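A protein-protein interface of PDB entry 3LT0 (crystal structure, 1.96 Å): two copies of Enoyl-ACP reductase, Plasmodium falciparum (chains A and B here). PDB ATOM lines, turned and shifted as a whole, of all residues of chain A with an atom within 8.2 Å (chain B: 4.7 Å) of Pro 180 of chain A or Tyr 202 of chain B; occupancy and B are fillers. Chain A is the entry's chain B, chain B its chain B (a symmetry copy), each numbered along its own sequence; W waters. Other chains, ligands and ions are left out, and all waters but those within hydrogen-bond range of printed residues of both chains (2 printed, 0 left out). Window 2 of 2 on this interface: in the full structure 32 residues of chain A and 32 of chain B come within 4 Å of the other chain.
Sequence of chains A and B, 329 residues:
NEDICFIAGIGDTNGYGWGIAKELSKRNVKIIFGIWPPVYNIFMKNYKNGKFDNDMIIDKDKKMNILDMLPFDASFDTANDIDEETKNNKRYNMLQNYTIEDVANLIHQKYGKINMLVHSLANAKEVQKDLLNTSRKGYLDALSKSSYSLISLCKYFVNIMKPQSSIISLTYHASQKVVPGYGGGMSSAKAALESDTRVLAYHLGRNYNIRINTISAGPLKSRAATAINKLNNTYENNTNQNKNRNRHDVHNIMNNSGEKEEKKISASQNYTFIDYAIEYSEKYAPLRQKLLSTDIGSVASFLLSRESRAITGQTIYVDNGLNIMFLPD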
ATOM      1  N   VAL A 127     -17.972 -17.660  -7.166  1.00  0.00           N
ATOM      2  CA  VAL A 127     -18.930 -17.761  -8.262  1.00  0.00           C
ATOM      3  C   VAL A 127     -18.713 -16.656  -9.309  1.00  0.00           C
ATOM      4  O   VAL A 127     -19.014 -16.841 -10.488  1.00  0.00           O
ATOM      5  CB  VAL A 127     -20.405 -17.798  -7.755  1.00  0.00           C
ATOM      6  CG1 VAL A 127     -20.780 -16.499  -7.009  1.00  0.00           C
ATOM      7  CG2 VAL A 127     -21.390 -18.116  -8.910  1.00  0.00           C
ATOM      8  N   ASP A 130     -14.491 -16.990 -13.540  1.00  0.00           N
ATOM      9  CA  ASP A 130     -14.673 -18.074 -14.499  1.00  0.00           C
ATOM     10  C   ASP A 130     -13.932 -19.296 -13.977  1.00  0.00           C
ATOM     11  O   ASP A 130     -12.984 -19.173 -13.190  1.00  0.00           O
ATOM     12  CB  ASP A 130     -14.180 -17.713 -15.904  1.00  0.00           C
ATOM     13  CG  ASP A 130     -12.698 -17.387 -15.943  1.00  0.00           C
ATOM     14  OD1 ASP A 130     -11.874 -18.203 -15.506  1.00  0.00           O
ATOM     15  OD2 ASP A 130     -12.353 -16.302 -16.419  1.00  0.00           O
ATOM     16  N   LEU A 131     -14.392 -20.466 -14.404  1.00  0.00           N
ATOM     17  CA  LEU A 131     -13.853 -21.763 -13.942  1.00  0.00           C
ATOM     18  C   LEU A 131     -12.333 -21.803 -14.000  1.00  0.00           C
ATOM     19  O   LEU A 131     -11.678 -22.219 -13.031  1.00  0.00           O
ATOM     20  CB  LEU A 131     -14.444 -22.938 -14.757  1.00  0.00           C
ATOM     21  CG  LEU A 131     -14.136 -24.353 -14.259  1.00  0.00           C
ATOM     22  CD1 LEU A 131     -14.755 -24.600 -12.886  1.00  0.00           C
ATOM     23  CD2 LEU A 131     -14.611 -25.445 -15.275  1.00  0.00           C
ATOM     24  N   LEU A 132     -11.766 -21.369 -15.131  1.00  0.00           N
ATOM     25  CA  LEU A 132     -10.323 -21.409 -15.364  1.00  0.00           C
ATOM     26  C   LEU A 132      -9.558 -20.632 -14.273  1.00  0.00           C
ATOM     27  O   LEU A 132      -8.432 -20.990 -13.941  1.00  0.00           O
ATOM     28  CB  LEU A 132     -10.006 -20.745 -16.709  1.00  0.00           C
ATOM     29  CG  LEU A 132      -8.958 -21.328 -17.658  1.00  0.00           C
ATOM     30  CD1 LEU A 132      -8.349 -20.232 -18.545  1.00  0.00           C
ATOM     31  CD2 LEU A 132      -7.898 -22.210 -16.989  1.00  0.00           C
ATOM     32  N   TYR A 172     -29.128 -26.730 -12.401  1.00  0.00           N
ATOM     33  CA  TYR A 172     -29.197 -25.808 -13.522  1.00  0.00           C
ATOM     34  C   TYR A 172     -28.421 -26.414 -14.701  1.00  0.00           C
ATOM     35  O   TYR A 172     -27.400 -27.124 -14.513  1.00  0.00           O
ATOM     36  CB  TYR A 172     -28.603 -24.426 -13.088  1.00  0.00           C
ATOM     37  CG  TYR A 172     -28.663 -23.375 -14.182  1.00  0.00           C
ATOM     38  CD1 TYR A 172     -29.881 -23.043 -14.806  1.00  0.00           C
ATOM     39  CD2 TYR A 172     -27.513 -22.710 -14.596  1.00  0.00           C
ATOM     40  CE1 TYR A 172     -29.935 -22.076 -15.844  1.00  0.00           C
ATOM     41  CE2 TYR A 172     -27.559 -21.722 -15.618  1.00  0.00           C
ATOM     42  CZ  TYR A 172     -28.763 -21.403 -16.212  1.00  0.00           C
ATOM     43  OH  TYR A 172     -28.765 -20.471 -17.240  1.00  0.00           O
ATOM     44  N   ALA A 174     -26.381 -25.348 -16.839  1.00  0.00           N
ATOM     45  CA  ALA A 174     -24.935 -25.078 -16.985  1.00  0.00           C
ATOM     46  C   ALA A 174     -24.066 -26.309 -16.691  1.00  0.00           C
ATOM     47  O   ALA A 174     -22.892 -26.296 -17.048  1.00  0.00           O
ATOM     48  CB  ALA A 174     -24.472 -23.909 -16.067  1.00  0.00           C
ATOM     49  N   LYS A 177     -24.428 -27.815 -20.539  1.00  0.00           N
ATOM     50  CA  LYS A 177     -24.048 -26.909 -21.628  1.00  0.00           C
ATOM     51  C   LYS A 177     -23.432 -25.645 -21.046  1.00  0.00           C
ATOM     52  O   LYS A 177     -23.765 -25.265 -19.942  1.00  0.00           O
ATOM     53  CB  LYS A 177     -25.250 -26.542 -22.494  1.00  0.00           C
ATOM     54  CG  LYS A 177     -25.944 -27.731 -23.133  1.00  0.00           C
ATOM     55  CD  LYS A 177     -25.078 -28.415 -24.187  1.00  0.00           C
ATOM     56  CE  LYS A 177     -25.886 -29.574 -24.862  1.00  0.00           C
ATOM     57  NZ  LYS A 177     -25.035 -30.361 -25.784  1.00  0.00           N
ATOM     58  N   VAL A 178     -22.541 -25.011 -21.792  1.00  0.00           N
ATOM     59  CA  VAL A 178     -21.746 -23.931 -21.264  1.00  0.00           C
ATOM     60  C   VAL A 178     -22.543 -22.655 -21.081  1.00  0.00           C
ATOM     61  O   VAL A 178     -23.212 -22.180 -22.011  1.00  0.00           O
ATOM     62  CB  VAL A 178     -20.488 -23.666 -22.125  1.00  0.00           C
ATOM     63  CG1 VAL A 178     -19.690 -22.464 -21.548  1.00  0.00           C
ATOM     64  CG2 VAL A 178     -19.621 -24.943 -22.154  1.00  0.00           C
ATOM     65  N   VAL A 179     -22.470 -22.134 -19.856  1.00  0.00           N
ATOM     66  CA  VAL A 179     -23.118 -20.872 -19.517  1.00  0.00           C
ATOM     67  C   VAL A 179     -22.041 -19.927 -18.964  1.00  0.00           C
ATOM     68  O   VAL A 179     -21.597 -20.061 -17.822  1.00  0.00           O
ATOM     69  CB  VAL A 179     -24.302 -21.030 -18.498  1.00  0.00           C
ATOM     70  CG1 VAL A 179     -24.811 -19.644 -18.022  1.00  0.00           C
ATOM     71  CG2 VAL A 179     -25.444 -21.834 -19.117  1.00  0.00           C
ATOM     72  N   PRO A 180     -21.598 -18.977 -19.790  1.00  0.00           N
ATOM     73  CA  PRO A 180     -20.619 -17.990 -19.313  1.00  0.00           C
ATOM     74  C   PRO A 180     -21.230 -17.185 -18.175  1.00  0.00           C
ATOM     75  O   PRO A 180     -22.392 -16.739 -18.267  1.00  0.00           O
ATOM     76  CB  PRO A 180     -20.391 -17.094 -20.541  1.00  0.00           C
ATOM     77  CG  PRO A 180     -20.668 -17.985 -21.686  1.00  0.00           C
ATOM     78  CD  PRO A 180     -21.817 -18.884 -21.240  1.00  0.00           C
ATOM     79  N   GLY A 181     -20.480 -17.018 -17.105  1.00  0.00           N
ATOM     80  CA  GLY A 181     -20.998 -16.282 -15.957  1.00  0.00           C
ATOM     81  C   GLY A 181     -21.338 -17.194 -14.798  1.00  0.00           C
ATOM     82  O   GLY A 181     -21.341 -16.767 -13.658  1.00  0.00           O
ATOM     83  N   TYR A 182     -21.607 -18.467 -15.073  1.00  0.00           N
ATOM     84  CA  TYR A 182     -21.940 -19.398 -13.990  1.00  0.00           C
ATOM     85  C   TYR A 182     -20.631 -19.993 -13.491  1.00  0.00           C
ATOM     86  O   TYR A 182     -20.245 -21.076 -13.891  1.00  0.00           O
ATOM     87  CB  TYR A 182     -22.905 -20.460 -14.526  1.00  0.00           C
ATOM     88  CG  TYR A 182     -23.701 -21.199 -13.466  1.00  0.00           C
ATOM     89  CD1 TYR A 182     -24.699 -20.550 -12.731  1.00  0.00           C
ATOM     90  CD2 TYR A 182     -23.501 -22.563 -13.244  1.00  0.00           C
ATOM     91  CE1 TYR A 182     -25.469 -21.255 -11.758  1.00  0.00           C
ATOM     92  CE2 TYR A 182     -24.244 -23.262 -12.279  1.00  0.00           C
ATOM     93  CZ  TYR A 182     -25.220 -22.607 -11.562  1.00  0.00           C
ATOM     94  OH  TYR A 182     -25.950 -23.316 -10.640  1.00  0.00           O
ATOM     95  N   GLY A 183     -19.914 -19.249 -12.646  1.00  0.00           N
ATOM     96  CA  GLY A 183     -18.511 -19.569 -12.381  1.00  0.00           C
ATOM     97  C   GLY A 183     -18.261 -20.188 -11.027  1.00  0.00           C
ATOM     98  O   GLY A 183     -19.172 -20.744 -10.395  1.00  0.00           O
ATOM     99  N   ILE A 228     -24.807 -13.095  -8.250  1.00  0.00           N
ATOM    100  CA  ILE A 228     -23.893 -13.556  -9.306  1.00  0.00           C
ATOM    101  C   ILE A 228     -23.389 -12.363 -10.131  1.00  0.00           C
ATOM    102  O   ILE A 228     -22.352 -12.453 -10.779  1.00  0.00           O
ATOM    103  CB  ILE A 228     -24.580 -14.587 -10.267  1.00  0.00           C
ATOM    104  CG1 ILE A 228     -24.928 -15.881  -9.521  1.00  0.00           C
ATOM    105  CG2 ILE A 228     -23.709 -14.891 -11.496  1.00  0.00           C
ATOM    106  CD1 ILE A 228     -25.777 -16.857 -10.323  1.00  0.00           C
ATOM    107  N   PHE A 273     -26.040 -10.739 -14.861  1.00  0.00           N
ATOM    108  CA  PHE A 273     -26.203 -12.139 -15.252  1.00  0.00           C
ATOM    109  C   PHE A 273     -27.682 -12.599 -15.278  1.00  0.00           C
ATOM    110  O   PHE A 273     -28.156 -13.072 -16.311  1.00  0.00           O
ATOM    111  CB  PHE A 273     -25.378 -13.077 -14.372  1.00  0.00           C
ATOM    112  CG  PHE A 273     -25.628 -14.524 -14.668  1.00  0.00           C
ATOM    113  CD1 PHE A 273     -24.987 -15.139 -15.737  1.00  0.00           C
ATOM    114  CD2 PHE A 273     -26.550 -15.260 -13.912  1.00  0.00           C
ATOM    115  CE1 PHE A 273     -25.241 -16.485 -16.032  1.00  0.00           C
ATOM    116  CE2 PHE A 273     -26.811 -16.598 -14.209  1.00  0.00           C
ATOM    117  CZ  PHE A 273     -26.160 -17.211 -15.259  1.00  0.00           C
ATOM    118  N   TYR A 276     -30.089 -10.940 -17.874  1.00  0.00           N
ATOM    119  CA  TYR A 276     -29.844 -11.444 -19.223  1.00  0.00           C
ATOM    120  C   TYR A 276     -30.511 -12.825 -19.390  1.00  0.00           C
ATOM    121  O   TYR A 276     -31.198 -13.072 -20.381  1.00  0.00           O
ATOM    122  CB  TYR A 276     -28.340 -11.558 -19.518  1.00  0.00           C
ATOM    123  CG  TYR A 276     -28.026 -12.213 -20.866  1.00  0.00           C
ATOM    124  CD1 TYR A 276     -28.143 -11.485 -22.063  1.00  0.00           C
ATOM    125  CD2 TYR A 276     -27.594 -13.551 -20.950  1.00  0.00           C
ATOM    126  CE1 TYR A 276     -27.854 -12.073 -23.305  1.00  0.00           C
ATOM    127  CE2 TYR A 276     -27.300 -14.140 -22.188  1.00  0.00           C
ATOM    128  CZ  TYR A 276     -27.437 -13.388 -23.360  1.00  0.00           C
ATOM    129  OH  TYR A 276     -27.160 -13.939 -24.595  1.00  0.00           O
ATOM    130  N   ALA A 277     -30.285 -13.700 -18.411  1.00  0.00           N
ATOM    131  CA  ALA A 277     -30.835 -15.067 -18.453  1.00  0.00           C
ATOM    132  C   ALA A 277     -32.354 -15.018 -18.608  1.00  0.00           C
ATOM    133  O   ALA A 277     -32.911 -15.737 -19.448  1.00  0.00           O
ATOM    134  CB  ALA A 277     -30.442 -15.842 -17.196  1.00  0.00           C
ATOM    135  N   ARG B 198     -16.134 -29.166 -21.039  1.00  0.00           N
ATOM    136  CA  ARG B 198     -16.912 -28.234 -21.861  1.00  0.00           C
ATOM    137  C   ARG B 198     -16.618 -26.771 -21.526  1.00  0.00           C
ATOM    138  O   ARG B 198     -16.336 -25.957 -22.418  1.00  0.00           O
ATOM    139  CB  ARG B 198     -18.417 -28.492 -21.689  1.00  0.00           C
ATOM    140  CG  ARG B 198     -18.883 -29.765 -22.314  1.00  0.00           C
ATOM    141  CD  ARG B 198     -20.401 -29.865 -22.125  1.00  0.00           C
ATOM    142  NE  ARG B 198     -20.826 -30.262 -20.779  1.00  0.00           N
ATOM    143  CZ  ARG B 198     -20.891 -31.529 -20.337  1.00  0.00           C
ATOM    144  NH1 ARG B 198     -20.500 -32.531 -21.099  1.00  0.00           N
ATOM    145  NH2 ARG B 198     -21.335 -31.804 -19.109  1.00  0.00           N
ATOM    146  N   VAL B 199     -16.679 -26.423 -20.242  1.00  0.00           N
ATOM    147  CA  VAL B 199     -16.476 -24.997 -19.830  1.00  0.00           C
ATOM    148  C   VAL B 199     -15.064 -24.536 -20.193  1.00  0.00           C
ATOM    149  O   VAL B 199     -14.888 -23.432 -20.726  1.00  0.00           O
ATOM    150  CB  VAL B 199     -16.772 -24.777 -18.315  1.00  0.00           C
ATOM    151  CG1 VAL B 199     -16.541 -23.321 -17.903  1.00  0.00           C
ATOM    152  CG2 VAL B 199     -18.222 -25.177 -18.037  1.00  0.00           C
ATOM    153  N   LEU B 200     -14.081 -25.394 -19.940  1.00  0.00           N
ATOM    154  CA  LEU B 200     -12.686 -25.123 -20.311  1.00  0.00           C
ATOM    155  C   LEU B 200     -12.524 -25.017 -21.825  1.00  0.00           C
ATOM    156  O   LEU B 200     -11.740 -24.206 -22.309  1.00  0.00           O
ATOM    157  CB  LEU B 200     -11.756 -26.194 -19.767  1.00  0.00           C
ATOM    158  CG  LEU B 200     -11.578 -26.229 -18.217  1.00  0.00           C
ATOM    159  CD1 LEU B 200     -10.830 -27.485 -17.807  1.00  0.00           C
ATOM    160  CD2 LEU B 200     -10.895 -24.978 -17.691  1.00  0.00           C
ATOM    161  N   ALA B 201     -13.273 -25.836 -22.573  1.00  0.00           N
ATOM    162  CA  ALA B 201     -13.193 -25.776 -24.032  1.00  0.00           C
ATOM    163  C   ALA B 201     -13.591 -24.386 -24.518  1.00  0.00           C
ATOM    164  O   ALA B 201     -13.005 -23.855 -25.471  1.00  0.00           O
ATOM    165  CB  ALA B 201     -14.069 -26.824 -24.680  1.00  0.00           C
ATOM    166  N   TYR B 202     -14.596 -23.823 -23.883  1.00  0.00           N
ATOM    167  CA  TYR B 202     -15.052 -22.467 -24.187  1.00  0.00           C
ATOM    168  C   TYR B 202     -13.959 -21.424 -23.901  1.00  0.00           C
ATOM    169  O   TYR B 202     -13.564 -20.722 -24.814  1.00  0.00           O
ATOM    170  CB  TYR B 202     -16.330 -22.157 -23.424  1.00  0.00           C
ATOM    171  CG  TYR B 202     -16.717 -20.694 -23.420  1.00  0.00           C
ATOM    172  CD1 TYR B 202     -17.170 -20.071 -24.582  1.00  0.00           C
ATOM    173  CD2 TYR B 202     -16.637 -19.946 -22.243  1.00  0.00           C
ATOM    174  CE1 TYR B 202     -17.539 -18.707 -24.570  1.00  0.00           C
ATOM    175  CE2 TYR B 202     -16.989 -18.600 -22.218  1.00  0.00           C
ATOM    176  CZ  TYR B 202     -17.439 -17.993 -23.385  1.00  0.00           C
ATOM    177  OH  TYR B 202     -17.784 -16.666 -23.331  1.00  0.00           O
ATOM    178  N   HIS B 203     -13.476 -21.339 -22.661  1.00  0.00           N
ATOM    179  CA  HIS B 203     -12.410 -20.393 -22.291  1.00  0.00           C
ATOM    180  C   HIS B 203     -11.100 -20.585 -23.083  1.00  0.00           C
ATOM    181  O   HIS B 203     -10.491 -19.616 -23.549  1.00  0.00           O
ATOM    182  CB  HIS B 203     -12.109 -20.399 -20.760  1.00  0.00           C
ATOM    183  CG  HIS B 203     -13.296 -20.104 -19.890  1.00  0.00           C
ATOM    184  ND1 HIS B 203     -13.943 -18.883 -19.893  1.00  0.00           N
ATOM    185  CD2 HIS B 203     -13.920 -20.852 -18.942  1.00  0.00           C
ATOM    186  CE1 HIS B 203     -14.953 -18.917 -19.043  1.00  0.00           C
ATOM    187  NE2 HIS B 203     -14.954 -20.095 -18.445  1.00  0.00           N
ATOM    188  N   LEU B 204     -10.643 -21.827 -23.214  1.00  0.00           N
ATOM    189  CA  LEU B 204      -9.361 -22.072 -23.871  1.00  0.00           C
ATOM    190  C   LEU B 204      -9.468 -21.883 -25.393  1.00  0.00           C
ATOM    191  O   LEU B 204      -8.503 -21.479 -26.045  1.00  0.00           O
ATOM    192  CB  LEU B 204      -8.830 -23.474 -23.561  1.00  0.00           C
ATOM    193  CG  LEU B 204      -8.575 -23.817 -22.090  1.00  0.00           C
ATOM    194  CD1 LEU B 204      -8.105 -25.286 -22.010  1.00  0.00           C
ATOM    195  CD2 LEU B 204      -7.524 -22.901 -21.528  1.00  0.00           C
ATOM    196  N   GLY B 205     -10.631 -22.219 -25.945  1.00  0.00           N
ATOM    197  CA  GLY B 205     -10.843 -22.093 -27.377  1.00  0.00           C
ATOM    198  C   GLY B 205     -10.885 -20.613 -27.737  1.00  0.00           C
ATOM    199  O   GLY B 205     -10.238 -20.191 -28.683  1.00  0.00           O
ATOM    200  N   ARG B 206     -11.651 -19.842 -26.988  1.00  0.00           N
ATOM    201  CA  ARG B 206     -11.828 -18.418 -27.286  1.00  0.00           C
ATOM    202  C   ARG B 206     -10.581 -17.586 -26.963  1.00  0.00           C
ATOM    203  O   ARG B 206     -10.207 -16.713 -27.747  1.00  0.00           O
ATOM    204  CB  ARG B 206     -13.033 -17.861 -26.539  1.00  0.00           C
ATOM    205  CG  ARG B 206     -14.398 -18.401 -27.023  1.00  0.00           C
ATOM    206  CD  ARG B 206     -14.805 -17.932 -28.424  1.00  0.00           C
ATOM    207  NE  ARG B 206     -16.244 -18.134 -28.587  1.00  0.00           N
ATOM    208  CZ  ARG B 206     -17.164 -17.334 -28.041  1.00  0.00           C
ATOM    209  NH1 ARG B 206     -16.791 -16.269 -27.347  1.00  0.00           N
ATOM    210  NH2 ARG B 206     -18.464 -17.577 -28.191  1.00  0.00           N
HETATM  211  O   HOH W   1     -21.001 -27.860 -19.093  1.00  0.00           O
HETATM  212  O   HOH W   2     -17.027 -20.251 -16.317  1.00  0.00           O
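Of the 17 printed residues of chain A, 4 touch a printed residue of chain B. Printed residues of chain A that touch a printed residue of chain B: Asp 130, Leu 131, Val 178 and Pro 180. Hydrophobic or aromatic side chains of chain A that line the printed part of chain B: Leu 131, Val 178 and Pro 180. Among the printed residues, 6 pairs touch across the chains.
Of the printed residues of chain B, Asp 130 of chain A touches His 203. Of the printed residues of chain B, Leu 131 of chain A touches Val 199. Printed residues of chain B within 4 Å of Val 178 of chain A: Arg 198 (3.4 Å), Val 199 (3.8 Å) and Tyr 202 (3.9 Å). Of the printed residues of chain A, Arg 198 of chain B touches Val 178. Of the printed residues of chain A, Val 199 of chain B touches Leu 131 and Val 178. No residue of chain A comes within 4 Å of Ala 201 of chain B. Of the printed residues of chain A, Tyr 202 of chain B touches Val 178 and Pro 180. The nearest printed residue of chain B that does not touch Pro 180 of chain A is His 203 of chain B (5.7 Å). The nearest residue of chain A that does not touch Tyr 202 of chain B is Val 179 of chain A (6.2 Å). The nearest printed residue of chain A that does not touch Arg 198 of chain B is Lys 177 of chain A (4.4 Å).
Among the printed residues, pairs that only touch across the chains: Val 178 of chain A with Arg 198 of chain B (3.4 Å), Asp 130 of chain A with His 203 of chain B (3.4 Å), Pro 180 of chain A with Tyr 202 of chain B (3.6 Å), Leu 131 of chain A with Val 199 of chain B (3.8 Å), Val 178 of chain A with Val 199 of chain B (3.8 Å) and Val 178 of chain A with Tyr 202 of chain B (3.9 Å).
No position is printed for both chains. Of the 6 pairs that touch across the chains among the printed residues, none has its exchanged pair printed and touching as well.
Water W1 bridges NE of Arg 198 of chain B and O of Ala 174 of chain A. Water W2 lies within hydrogen-bond range of a ring nitrogen (NE2) of His 203 of chain B (3.0 Å) and the backbone NH (N) of Leu 131 of chain A (3.3 Å).
The side-chain carboxylate of Asp 130 of chain A sits at hydrogen-bond distance from the backbone NH of Leu 132 of chain A, at 3.2 Å.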
